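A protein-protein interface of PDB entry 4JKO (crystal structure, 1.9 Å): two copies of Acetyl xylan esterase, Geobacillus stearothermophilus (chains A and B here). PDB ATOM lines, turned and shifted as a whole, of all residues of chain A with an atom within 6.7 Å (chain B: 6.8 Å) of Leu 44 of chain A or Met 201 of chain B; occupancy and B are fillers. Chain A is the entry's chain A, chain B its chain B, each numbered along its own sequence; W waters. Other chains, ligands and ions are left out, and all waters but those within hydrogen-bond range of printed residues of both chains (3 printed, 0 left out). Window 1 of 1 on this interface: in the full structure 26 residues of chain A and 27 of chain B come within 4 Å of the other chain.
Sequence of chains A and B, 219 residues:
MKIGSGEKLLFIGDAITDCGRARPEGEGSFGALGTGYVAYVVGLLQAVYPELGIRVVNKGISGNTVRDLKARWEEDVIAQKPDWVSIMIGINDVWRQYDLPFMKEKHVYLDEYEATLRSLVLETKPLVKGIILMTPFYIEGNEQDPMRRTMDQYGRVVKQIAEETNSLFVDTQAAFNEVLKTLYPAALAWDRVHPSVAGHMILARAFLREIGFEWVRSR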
ATOM      1  N   ALA A  39      13.527  29.598   7.039  1.00  0.00           N
ATOM      2  CA  ALA A  39      13.415  28.152   7.322  1.00  0.00           C
ATOM      3  C   ALA A  39      12.837  27.841   8.689  1.00  0.00           C
ATOM      4  O   ALA A  39      12.042  26.877   8.820  1.00  0.00           O
ATOM      5  CB  ALA A  39      14.782  27.537   7.171  1.00  0.00           C
ATOM      6  N   TYR A  40      13.119  28.674   9.678  1.00  0.00           N
ATOM      7  CA  TYR A  40      12.609  28.448  10.992  1.00  0.00           C
ATOM      8  C   TYR A  40      11.111  28.674  11.003  1.00  0.00           C
ATOM      9  O   TYR A  40      10.390  27.921  11.634  1.00  0.00           O
ATOM     10  CB  TYR A  40      13.258  29.338  12.049  1.00  0.00           C
ATOM     11  CG  TYR A  40      14.792  29.182  12.181  1.00  0.00           C
ATOM     12  CD1 TYR A  40      15.464  28.085  11.641  1.00  0.00           C
ATOM     13  CD2 TYR A  40      15.469  30.038  12.936  1.00  0.00           C
ATOM     14  CE1 TYR A  40      16.844  27.943  11.837  1.00  0.00           C
ATOM     15  CE2 TYR A  40      16.819  29.945  13.134  1.00  0.00           C
ATOM     16  CZ  TYR A  40      17.508  28.897  12.570  1.00  0.00           C
ATOM     17  OH  TYR A  40      18.830  28.831  12.775  1.00  0.00           O
ATOM     18  N   VAL A  41      10.641  29.736  10.345  1.00  0.00           N
ATOM     19  CA  VAL A  41       9.177  29.943  10.254  1.00  0.00           C
ATOM     20  C   VAL A  41       8.495  28.741   9.632  1.00  0.00           C
ATOM     21  O   VAL A  41       7.458  28.240  10.104  1.00  0.00           O
ATOM     22  CB  VAL A  41       8.931  31.232   9.406  1.00  0.00           C
ATOM     23  CG1 VAL A  41       7.466  31.292   8.975  1.00  0.00           C
ATOM     24  CG2 VAL A  41       9.352  32.502  10.177  1.00  0.00           C
ATOM     25  N   VAL A  42       9.054  28.248   8.535  1.00  0.00           N
ATOM     26  CA  VAL A  42       8.445  27.106   7.804  1.00  0.00           C
ATOM     27  C   VAL A  42       8.463  25.869   8.673  1.00  0.00           C
ATOM     28  O   VAL A  42       7.454  25.166   8.783  1.00  0.00           O
ATOM     29  CB  VAL A  42       9.097  26.869   6.445  1.00  0.00           C
ATOM     30  CG1 VAL A  42       8.396  25.737   5.677  1.00  0.00           C
ATOM     31  CG2 VAL A  42       9.011  28.126   5.591  1.00  0.00           C
ATOM     32  N   GLY A  43       9.572  25.643   9.377  1.00  0.00           N
ATOM     33  CA  GLY A  43       9.638  24.582  10.331  1.00  0.00           C
ATOM     34  C   GLY A  43       8.661  24.631  11.456  1.00  0.00           C
ATOM     35  O   GLY A  43       8.058  23.645  11.811  1.00  0.00           O
ATOM     36  N   LEU A  44       8.500  25.795  12.046  1.00  0.00           N
ATOM     37  CA  LEU A  44       7.565  25.907  13.123  1.00  0.00           C
ATOM     38  C   LEU A  44       6.134  25.766  12.608  1.00  0.00           C
ATOM     39  O   LEU A  44       5.278  25.211  13.290  1.00  0.00           O
ATOM     40  CB  LEU A  44       7.782  27.203  13.897  1.00  0.00           C
ATOM     41  CG  LEU A  44       8.992  27.108  14.850  1.00  0.00           C
ATOM     42  CD1 LEU A  44       9.421  28.445  15.326  1.00  0.00           C
ATOM     43  CD2 LEU A  44       8.585  26.257  16.027  1.00  0.00           C
ATOM     44  N   LEU A  45       5.853  26.279  11.423  1.00  0.00           N
ATOM     45  CA  LEU A  45       4.475  26.123  10.923  1.00  0.00           C
ATOM     46  C   LEU A  45       4.143  24.665  10.659  1.00  0.00           C
ATOM     47  O   LEU A  45       3.017  24.209  10.891  1.00  0.00           O
ATOM     48  CB  LEU A  45       4.265  26.979   9.672  1.00  0.00           C
ATOM     49  CG  LEU A  45       4.212  28.452   9.960  1.00  0.00           C
ATOM     50  CD1 LEU A  45       4.209  29.236   8.657  1.00  0.00           C
ATOM     51  CD2 LEU A  45       2.901  28.670  10.713  1.00  0.00           C
ATOM     52  N   GLN A  46       5.128  23.942  10.138  1.00  0.00           N
ATOM     53  CA  GLN A  46       4.935  22.557   9.857  1.00  0.00           C
ATOM     54  C   GLN A  46       4.828  21.739  11.138  1.00  0.00           C
ATOM     55  O   GLN A  46       4.068  20.776  11.183  1.00  0.00           O
ATOM     56  CB  GLN A  46       6.000  22.019   8.953  1.00  0.00           C
ATOM     57  CG  GLN A  46       5.662  20.604   8.533  1.00  0.00           C
ATOM     58  CD  GLN A  46       6.366  20.198   7.256  1.00  0.00           C
ATOM     59  OE1 GLN A  46       7.516  19.771   7.270  1.00  0.00           O
ATOM     60  NE2 GLN A  46       5.642  20.278   6.136  1.00  0.00           N
ATOM     61  N   ALA A  47       5.546  22.132  12.168  1.00  0.00           N
ATOM     62  CA  ALA A  47       5.546  21.390  13.424  1.00  0.00           C
ATOM     63  C   ALA A  47       4.235  21.553  14.157  1.00  0.00           C
ATOM     64  O   ALA A  47       3.834  20.685  14.931  1.00  0.00           O
ATOM     65  CB  ALA A  47       6.613  21.943  14.339  1.00  0.00           C
ATOM     66  N   VAL A  48       3.661  22.757  14.052  1.00  0.00           N
ATOM     67  CA  VAL A  48       2.486  23.055  14.839  1.00  0.00           C
ATOM     68  C   VAL A  48       1.154  23.096  14.040  1.00  0.00           C
ATOM     69  O   VAL A  48       0.090  22.776  14.570  1.00  0.00           O
ATOM     70  CB  VAL A  48       2.728  24.389  15.574  1.00  0.00           C
ATOM     71  CG1 VAL A  48       1.469  24.735  16.374  1.00  0.00           C
ATOM     72  CG2 VAL A  48       3.977  24.294  16.432  1.00  0.00           C
ATOM     73  N   TYR A  49       1.270  23.464  12.760  1.00  0.00           N
ATOM     74  CA  TYR A  49       0.204  23.375  11.768  1.00  0.00           C
ATOM     75  C   TYR A  49       0.524  22.573  10.512  1.00  0.00           C
ATOM     76  O   TYR A  49       0.471  23.090   9.413  1.00  0.00           O
ATOM     77  CB  TYR A  49      -0.093  24.802  11.298  1.00  0.00           C
ATOM     78  CG  TYR A  49      -0.413  25.778  12.412  1.00  0.00           C
ATOM     79  CD1 TYR A  49      -1.739  26.171  12.653  1.00  0.00           C
ATOM     80  CD2 TYR A  49       0.593  26.370  13.202  1.00  0.00           C
ATOM     81  CE1 TYR A  49      -2.040  27.105  13.627  1.00  0.00           C
ATOM     82  CE2 TYR A  49       0.287  27.300  14.194  1.00  0.00           C
ATOM     83  CZ  TYR A  49      -1.056  27.654  14.392  1.00  0.00           C
ATOM     84  OH  TYR A  49      -1.394  28.563  15.346  1.00  0.00           O
ATOM     85  N   PRO A  50       0.862  21.300  10.671  1.00  0.00           N
ATOM     86  CA  PRO A  50       1.221  20.479   9.538  1.00  0.00           C
ATOM     87  C   PRO A  50       0.131  20.396   8.497  1.00  0.00           C
ATOM     88  O   PRO A  50       0.399  20.463   7.306  1.00  0.00           O
ATOM     89  CB  PRO A  50       1.521  19.131  10.192  1.00  0.00           C
ATOM     90  CG  PRO A  50       0.858  19.118  11.500  1.00  0.00           C
ATOM     91  CD  PRO A  50       0.864  20.562  11.948  1.00  0.00           C
ATOM     92  N   MET A 201      16.022  33.352  15.318  1.00  0.00           N
ATOM     93  CA  MET A 201      14.803  32.982  16.118  1.00  0.00           C
ATOM     94  C   MET A 201      14.010  34.201  16.570  1.00  0.00           C
ATOM     95  O   MET A 201      12.776  34.164  16.598  1.00  0.00           O
ATOM     96  CB  MET A 201      15.194  32.168  17.365  1.00  0.00           C
ATOM     97  CG  MET A 201      15.525  30.734  17.007  1.00  0.00           C
ATOM     98  SD  MET A 201      14.147  29.776  16.384  1.00  0.00           S
ATOM     99  CE  MET A 201      14.988  28.250  16.081  1.00  0.00           C
ATOM    100  N   ALA A 204      12.130  35.096  13.401  1.00  0.00           N
ATOM    101  CA  ALA A 204      11.098  34.110  13.127  1.00  0.00           C
ATOM    102  C   ALA A 204       9.890  34.228  14.128  1.00  0.00           C
ATOM    103  O   ALA A 204       8.705  34.187  13.718  1.00  0.00           O
ATOM    104  CB  ALA A 204      11.704  32.697  13.177  1.00  0.00           C
ATOM    105  N   ARG A 205      10.206  34.416  15.378  1.00  0.00           N
ATOM    106  CA  ARG A 205       9.184  34.620  16.376  1.00  0.00           C
ATOM    107  C   ARG A 205       8.471  35.939  16.122  1.00  0.00           C
ATOM    108  O   ARG A 205       7.245  35.985  16.243  1.00  0.00           O
ATOM    109  CB  ARG A 205       9.782  34.573  17.742  1.00  0.00           C
ATOM    110  CG  ARG A 205       8.849  34.827  18.851  1.00  0.00           C
ATOM    111  CD  ARG A 205       9.522  34.430  20.128  1.00  0.00           C
ATOM    112  NE  ARG A 205       8.878  34.771  21.392  1.00  0.00           N
ATOM    113  CZ  ARG A 205       9.084  35.900  22.057  1.00  0.00           C
ATOM    114  NH1 ARG A 205       9.816  36.870  21.534  1.00  0.00           N
ATOM    115  NH2 ARG A 205       8.519  36.083  23.224  1.00  0.00           N
ATOM    116  N   LEU A 208       6.020  35.246  13.282  1.00  0.00           N
ATOM    117  CA  LEU A 208       4.980  34.291  13.603  1.00  0.00           C
ATOM    118  C   LEU A 208       3.927  34.946  14.492  1.00  0.00           C
ATOM    119  O   LEU A 208       2.712  34.669  14.356  1.00  0.00           O
ATOM    120  CB  LEU A 208       5.629  33.048  14.321  1.00  0.00           C
ATOM    121  CG  LEU A 208       6.278  32.105  13.298  1.00  0.00           C
ATOM    122  CD1 LEU A 208       7.111  31.057  14.017  1.00  0.00           C
ATOM    123  CD2 LEU A 208       5.256  31.419  12.427  1.00  0.00           C
ATOM    124  N   PHE A 213       0.364  32.991  14.873  1.00  0.00           N
ATOM    125  CA  PHE A 213       0.853  31.640  15.251  1.00  0.00           C
ATOM    126  C   PHE A 213       0.633  31.404  16.710  1.00  0.00           C
ATOM    127  O   PHE A 213       0.797  32.294  17.533  1.00  0.00           O
ATOM    128  CB  PHE A 213       2.362  31.572  14.941  1.00  0.00           C
ATOM    129  CG  PHE A 213       3.088  30.358  15.488  1.00  0.00           C
ATOM    130  CD1 PHE A 213       3.213  29.240  14.729  1.00  0.00           C
ATOM    131  CD2 PHE A 213       3.734  30.424  16.695  1.00  0.00           C
ATOM    132  CE1 PHE A 213       3.950  28.161  15.156  1.00  0.00           C
ATOM    133  CE2 PHE A 213       4.459  29.330  17.184  1.00  0.00           C
ATOM    134  CZ  PHE A 213       4.564  28.184  16.390  1.00  0.00           C
ATOM    135  N   TRP A 215       2.035  28.865  19.738  1.00  0.00           N
ATOM    136  CA  TRP A 215       3.014  27.839  20.126  1.00  0.00           C
ATOM    137  C   TRP A 215       2.342  26.505  20.499  1.00  0.00           C
ATOM    138  O   TRP A 215       2.774  25.434  20.089  1.00  0.00           O
ATOM    139  CB  TRP A 215       3.817  28.380  21.307  1.00  0.00           C
ATOM    140  CG  TRP A 215       4.860  27.446  21.899  1.00  0.00           C
ATOM    141  CD1 TRP A 215       4.829  26.859  23.111  1.00  0.00           C
ATOM    142  CD2 TRP A 215       6.118  27.070  21.304  1.00  0.00           C
ATOM    143  NE1 TRP A 215       5.971  26.060  23.297  1.00  0.00           N
ATOM    144  CE2 TRP A 215       6.785  26.213  22.223  1.00  0.00           C
ATOM    145  CE3 TRP A 215       6.739  27.369  20.088  1.00  0.00           C
ATOM    146  CZ2 TRP A 215       8.049  25.686  21.968  1.00  0.00           C
ATOM    147  CZ3 TRP A 215       7.999  26.839  19.814  1.00  0.00           C
ATOM    148  CH2 TRP A 215       8.651  26.018  20.772  1.00  0.00           C
ATOM    149  N   GLY B  36      20.823  21.597  14.364  1.00  0.00           N
ATOM    150  CA  GLY B  36      19.547  20.945  14.598  1.00  0.00           C
ATOM    151  C   GLY B  36      18.901  21.350  15.868  1.00  0.00           C
ATOM    152  O   GLY B  36      19.008  22.504  16.346  1.00  0.00           O
ATOM    153  N   TYR B  37      18.190  20.395  16.481  1.00  0.00           N
ATOM    154  CA  TYR B  37      17.353  20.749  17.593  1.00  0.00           C
ATOM    155  C   TYR B  37      18.076  21.338  18.752  1.00  0.00           C
ATOM    156  O   TYR B  37      17.514  22.187  19.441  1.00  0.00           O
ATOM    157  CB  TYR B  37      16.385  19.583  18.063  1.00  0.00           C
ATOM    158  CG  TYR B  37      17.047  18.595  19.014  1.00  0.00           C
ATOM    159  CD1 TYR B  37      17.052  18.814  20.366  1.00  0.00           C
ATOM    160  CD2 TYR B  37      17.744  17.517  18.539  1.00  0.00           C
ATOM    161  CE1 TYR B  37      17.684  17.927  21.251  1.00  0.00           C
ATOM    162  CE2 TYR B  37      18.371  16.582  19.420  1.00  0.00           C
ATOM    163  CZ  TYR B  37      18.331  16.802  20.761  1.00  0.00           C
ATOM    164  OH  TYR B  37      18.990  15.957  21.616  1.00  0.00           O
ATOM    165  N   TYR B  40      18.527  24.912  17.939  1.00  0.00           N
ATOM    166  CA  TYR B  40      17.202  25.588  18.007  1.00  0.00           C
ATOM    167  C   TYR B  40      16.781  25.877  19.454  1.00  0.00           C
ATOM    168  O   TYR B  40      16.276  26.965  19.760  1.00  0.00           O
ATOM    169  CB  TYR B  40      16.187  24.798  17.280  1.00  0.00           C
ATOM    170  CG  TYR B  40      16.440  24.582  15.822  1.00  0.00           C
ATOM    171  CD1 TYR B  40      17.464  25.231  15.121  1.00  0.00           C
ATOM    172  CD2 TYR B  40      15.687  23.706  15.124  1.00  0.00           C
ATOM    173  CE1 TYR B  40      17.649  25.001  13.771  1.00  0.00           C
ATOM    174  CE2 TYR B  40      15.872  23.480  13.774  1.00  0.00           C
ATOM    175  CZ  TYR B  40      16.857  24.112  13.113  1.00  0.00           C
ATOM    176  OH  TYR B  40      17.054  23.827  11.805  1.00  0.00           O
ATOM    177  N   LEU B  44      16.077  29.646  20.877  1.00  0.00           N
ATOM    178  CA  LEU B  44      14.837  30.063  21.480  1.00  0.00           C
ATOM    179  C   LEU B  44      15.044  30.482  22.933  1.00  0.00           C
ATOM    180  O   LEU B  44      14.484  31.466  23.351  1.00  0.00           O
ATOM    181  CB  LEU B  44      13.794  28.954  21.431  1.00  0.00           C
ATOM    182  CG  LEU B  44      13.197  28.922  20.022  1.00  0.00           C
ATOM    183  CD1 LEU B  44      12.535  27.624  19.673  1.00  0.00           C
ATOM    184  CD2 LEU B  44      12.250  30.104  19.786  1.00  0.00           C
ATOM    185  N   SER B 196      14.104  17.042   8.379  1.00  0.00           N
ATOM    186  CA  SER B 196      14.197  18.385   7.877  1.00  0.00           C
ATOM    187  C   SER B 196      14.310  19.338   9.066  1.00  0.00           C
ATOM    188  O   SER B 196      14.127  18.918  10.256  1.00  0.00           O
ATOM    189  CB  SER B 196      12.881  18.711   7.124  1.00  0.00           C
ATOM    190  OG  SER B 196      11.789  18.605   8.015  1.00  0.00           O
ATOM    191  N   VAL B 197      14.509  20.625   8.784  1.00  0.00           N
ATOM    192  CA  VAL B 197      14.328  21.675   9.828  1.00  0.00           C
ATOM    193  C   VAL B 197      13.023  21.454  10.601  1.00  0.00           C
ATOM    194  O   VAL B 197      12.971  21.669  11.827  1.00  0.00           O
ATOM    195  CB  VAL B 197      14.406  23.083   9.214  1.00  0.00           C
ATOM    196  CG1 VAL B 197      14.022  24.211  10.201  1.00  0.00           C
ATOM    197  CG2 VAL B 197      15.809  23.345   8.569  1.00  0.00           C
ATOM    198  N   ALA B 198      11.951  21.122   9.900  1.00  0.00           N
ATOM    199  CA  ALA B 198      10.659  20.943  10.575  1.00  0.00           C
ATOM    200  C   ALA B 198      10.787  19.859  11.638  1.00  0.00           C
ATOM    201  O   ALA B 198      10.284  20.011  12.749  1.00  0.00           O
ATOM    202  CB  ALA B 198       9.534  20.589   9.598  1.00  0.00           C
ATOM    203  N   GLY B 199      11.455  18.737  11.308  1.00  0.00           N
ATOM    204  CA  GLY B 199      11.615  17.694  12.295  1.00  0.00           C
ATOM    205  C   GLY B 199      12.420  18.082  13.499  1.00  0.00           C
ATOM    206  O   GLY B 199      12.113  17.687  14.641  1.00  0.00           O
ATOM    207  N   HIS B 200      13.488  18.867  13.272  1.00  0.00           N
ATOM    208  CA  HIS B 200      14.278  19.413  14.352  1.00  0.00           C
ATOM    209  C   HIS B 200      13.482  20.397  15.177  1.00  0.00           C
ATOM    210  O   HIS B 200      13.638  20.522  16.399  1.00  0.00           O
ATOM    211  CB  HIS B 200      15.668  19.919  13.874  1.00  0.00           C
ATOM    212  CG  HIS B 200      16.645  18.811  13.701  1.00  0.00           C
ATOM    213  ND1 HIS B 200      16.853  18.156  12.491  1.00  0.00           N
ATOM    214  CD2 HIS B 200      17.374  18.137  14.615  1.00  0.00           C
ATOM    215  CE1 HIS B 200      17.717  17.170  12.676  1.00  0.00           C
ATOM    216  NE2 HIS B 200      18.053  17.151  13.943  1.00  0.00           N
ATOM    217  N   MET B 201      12.578  21.112  14.519  1.00  0.00           N
ATOM    218  CA  MET B 201      11.708  21.939  15.262  1.00  0.00           C
ATOM    219  C   MET B 201      10.706  21.171  16.123  1.00  0.00           C
ATOM    220  O   MET B 201      10.396  21.615  17.238  1.00  0.00           O
ATOM    221  CB  MET B 201      10.889  22.895  14.354  1.00  0.00           C
ATOM    222  CG  MET B 201      11.621  24.105  13.968  1.00  0.00           C
ATOM    223  SD  MET B 201      12.210  25.223  15.262  1.00  0.00           S
ATOM    224  CE  MET B 201      12.869  26.412  14.093  1.00  0.00           C
ATOM    225  N   ILE B 202      10.170  20.098  15.594  1.00  0.00           N
ATOM    226  CA  ILE B 202       9.261  19.207  16.362  1.00  0.00           C
ATOM    227  C   ILE B 202      10.013  18.769  17.624  1.00  0.00           C
ATOM    228  O   ILE B 202       9.476  18.776  18.742  1.00  0.00           O
ATOM    229  CB  ILE B 202       8.812  17.990  15.570  1.00  0.00           C
ATOM    230  CG1 ILE B 202       7.798  18.421  14.479  1.00  0.00           C
ATOM    231  CG2 ILE B 202       8.156  16.932  16.486  1.00  0.00           C
ATOM    232  CD1 ILE B 202       7.579  17.395  13.365  1.00  0.00           C
ATOM    233  N   LEU B 203      11.291  18.427  17.449  1.00  0.00           N
ATOM    234  CA  LEU B 203      12.086  17.983  18.644  1.00  0.00           C
ATOM    235  C   LEU B 203      12.338  19.083  19.597  1.00  0.00           C
ATOM    236  O   LEU B 203      12.176  18.920  20.809  1.00  0.00           O
ATOM    237  CB  LEU B 203      13.428  17.438  18.214  1.00  0.00           C
ATOM    238  CG  LEU B 203      13.261  16.122  17.426  1.00  0.00           C
ATOM    239  CD1 LEU B 203      14.516  15.735  16.713  1.00  0.00           C
ATOM    240  CD2 LEU B 203      12.955  15.035  18.392  1.00  0.00           C
ATOM    241  N   ALA B 204      12.832  20.208  19.079  1.00  0.00           N
ATOM    242  CA  ALA B 204      13.111  21.348  19.948  1.00  0.00           C
ATOM    243  C   ALA B 204      11.904  21.764  20.761  1.00  0.00           C
ATOM    244  O   ALA B 204      11.996  22.088  21.953  1.00  0.00           O
ATOM    245  CB  ALA B 204      13.582  22.528  19.136  1.00  0.00           C
ATOM    246  N   ARG B 205      10.795  21.890  20.070  1.00  0.00           N
ATOM    247  CA  ARG B 205       9.553  22.251  20.749  1.00  0.00           C
ATOM    248  C   ARG B 205       9.134  21.270  21.814  1.00  0.00           C
ATOM    249  O   ARG B 205       8.743  21.659  22.912  1.00  0.00           O
ATOM    250  CB  ARG B 205       8.447  22.424  19.764  1.00  0.00           C
ATOM    251  CG  ARG B 205       7.103  22.754  20.418  1.00  0.00           C
ATOM    252  CD  ARG B 205       6.245  23.319  19.314  1.00  0.00           C
ATOM    253  NE  ARG B 205       4.833  23.424  19.670  1.00  0.00           N
ATOM    254  CZ  ARG B 205       3.928  22.472  19.488  1.00  0.00           C
ATOM    255  NH1 ARG B 205       4.247  21.213  19.076  1.00  0.00           N
ATOM    256  NH2 ARG B 205       2.648  22.770  19.751  1.00  0.00           N
ATOM    257  N   ALA B 206       9.335  20.009  21.538  1.00  0.00           N
ATOM    258  CA  ALA B 206       8.939  18.977  22.513  1.00  0.00           C
ATOM    259  C   ALA B 206       9.833  19.067  23.742  1.00  0.00           C
ATOM    260  O   ALA B 206       9.362  18.859  24.832  1.00  0.00           O
ATOM    261  CB  ALA B 206       9.033  17.601  21.884  1.00  0.00           C
ATOM    262  N   PHE B 207      11.137  19.374  23.559  1.00  0.00           N
ATOM    263  CA  PHE B 207      12.022  19.513  24.653  1.00  0.00           C
ATOM    264  C   PHE B 207      11.600  20.741  25.491  1.00  0.00           C
ATOM    265  O   PHE B 207      11.596  20.736  26.743  1.00  0.00           O
ATOM    266  CB  PHE B 207      13.471  19.697  24.155  1.00  0.00           C
ATOM    267  CG  PHE B 207      14.443  19.893  25.241  1.00  0.00           C
ATOM    268  CD1 PHE B 207      15.057  18.807  25.831  1.00  0.00           C
ATOM    269  CD2 PHE B 207      14.760  21.197  25.691  1.00  0.00           C
ATOM    270  CE1 PHE B 207      15.939  19.016  26.872  1.00  0.00           C
ATOM    271  CE2 PHE B 207      15.682  21.392  26.685  1.00  0.00           C
ATOM    272  CZ  PHE B 207      16.261  20.288  27.280  1.00  0.00           C
ATOM    273  N   LEU B 208      11.368  21.821  24.783  1.00  0.00           N
ATOM    274  CA  LEU B 208      11.120  23.137  25.446  1.00  0.00           C
ATOM    275  C   LEU B 208       9.846  23.059  26.304  1.00  0.00           C
ATOM    276  O   LEU B 208       9.827  23.568  27.424  1.00  0.00           O
ATOM    277  CB  LEU B 208      10.994  24.173  24.372  1.00  0.00           C
ATOM    278  CG  LEU B 208      12.375  24.633  23.827  1.00  0.00           C
ATOM    279  CD1 LEU B 208      12.199  25.405  22.561  1.00  0.00           C
ATOM    280  CD2 LEU B 208      13.229  25.415  24.821  1.00  0.00           C
ATOM    281  N   TRP B 215       6.453  30.540  25.151  1.00  0.00           N
ATOM    282  CA  TRP B 215       6.702  31.236  23.939  1.00  0.00           C
ATOM    283  C   TRP B 215       6.568  32.759  24.106  1.00  0.00           C
ATOM    284  O   TRP B 215       7.381  33.523  23.552  1.00  0.00           O
ATOM    285  CB  TRP B 215       5.713  30.761  22.928  1.00  0.00           C
ATOM    286  CG  TRP B 215       5.668  31.447  21.586  1.00  0.00           C
ATOM    287  CD1 TRP B 215       4.645  32.231  21.125  1.00  0.00           C
ATOM    288  CD2 TRP B 215       6.575  31.278  20.474  1.00  0.00           C
ATOM    289  NE1 TRP B 215       4.896  32.622  19.826  1.00  0.00           N
ATOM    290  CE2 TRP B 215       6.057  32.038  19.400  1.00  0.00           C
ATOM    291  CE3 TRP B 215       7.786  30.570  20.292  1.00  0.00           C
ATOM    292  CZ2 TRP B 215       6.688  32.123  18.183  1.00  0.00           C
ATOM    293  CZ3 TRP B 215       8.392  30.614  19.067  1.00  0.00           C
ATOM    294  CH2 TRP B 215       7.855  31.408  18.029  1.00  0.00           C
HETATM  295  O   HOH W   1       5.121  19.009  16.811  1.00  0.00           O
HETATM  296  O   HOH W   2       9.591  18.742   6.520  1.00  0.00           O
HETATM  297  O   HOH W   3       2.595  33.684  18.717  1.00  0.00           O
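O of Trp 215 of chain B lies within hydrogen-bond range of NH2 of Arg 205 of chain A (2.8 Å). NH2 of Arg 205 of chain B sits at hydrogen-bond distance from O of Trp 215 of chain A (2.7 Å).
The backbone NH of Ala 198 of chain B lies close to the side-chain hydroxyl of Ser 196 of chain B. The backbone carbonyl oxygen (O) of Leu 208 of chain A sits at hydrogen-bond distance from the backbone NH (N) of Phe 213 of chain A (2.9 Å).
Among the printed residues, merely in contact across the chains: Ala 39 of chain A with Val 197 of chain B (3.6 Å), Tyr 40 of chain A with Tyr 40 of chain B (3.6 Å), Tyr 40 of chain A with Met 201 of chain B (3.6 Å), Gly 43 of chain A with Ala 198 of chain B (3.8 Å), Gly 43 of chain A with Met 201 of chain B (3.9 Å), Leu 44 of chain A with Met 201 of chain B (3.8 Å), Gln 46 of chain A with Ala 198 of chain B (3.2 Å), Ala 47 of chain A with Ile 202 of chain B (3.7 Å), Val 48 of chain A with Arg 205 of chain B (3.5 Å), Met 201 of chain A with Tyr 40 of chain B (3.8 Å), Met 201 of chain A with Leu 44 of chain B (3.9 Å), Met 201 of chain A with Met 201 of chain B (3.4 Å), Phe 213 of chain A with Trp 215 of chain B (3.7 Å) and Trp 215 of chain A with Trp 215 of chain B (3.4 Å).
Of the printed residues of chain B, Gln 46 of chain A touches Ala 198. Printed residues of chain B within 4 Å of Arg 205 of chain A: Trp 215 (2.8 Å). Printed residues of chain A within 4 Å of Leu 44 of chain B: Met 201 (3.9 Å). Of the printed residues of chain A, Val 197 of chain B touches Ala 39 (3.6 Å). Met 201 of chain B touches just these residues of chain A: Tyr 40, Gly 43, Leu 44 and Met 201. The nearest residue of chain A that does not touch Met 201 of chain B is Ala 47 of chain A (4.4 Å). The nearest printed residue of chain B that does not touch Ala 47 of chain A is Arg 205 of chain B (4.2 Å).
Hydrophobic or aromatic side chains of chain A that line the printed part of chain B: Tyr 40, Leu 44, Ala 47, Val 48, Met 201, Phe 213 and Trp 215. Hydrophobic or aromatic side chains of chain B within 4 Å of the printed part of chain A: Tyr 40, Leu 44, Val 197, Ala 198, Met 201, Ile 202 and Trp 215. Among the printed residues, 16 pairs touch across the chains.
Tyr 40 of chain A touches Met 201 of chain B, and with the chains exchanged Met 201 of chain A touches Tyr 40 of chain B. Met 201 of chain A touches its own counterpart, Met 201 of chain B. Arg 205 of chain A touches Trp 215 of chain B, and with the chains exchanged Trp 215 of chain A touches Arg 205 of chain B. Trp 215 of chain A touches its own counterpart, Trp 215 of chain B. 7 positions are printed for both chains. Of the 16 pairs that touch across the chains among the printed residues, 9 have their exchanged pair printed and touching as well.
Water W2 lies within hydrogen-bond range of the side-chain amide oxygen of Gln 46 of chain A and the side-chain hydroxyl of Ser 196 of chain B. Water W3 lies within hydrogen-bond range of the backbone carbonyl oxygen (O) of Phe 213 of chain A (2.6 Å) and the indole nitrogen (NE1) of Trp 215 of chain B (2.8 Å). Water W1 lies within hydrogen-bond range of O of Ala 47 of chain A (2.8 Å) and NH1 of Arg 205 of chain B (3.3 Å).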
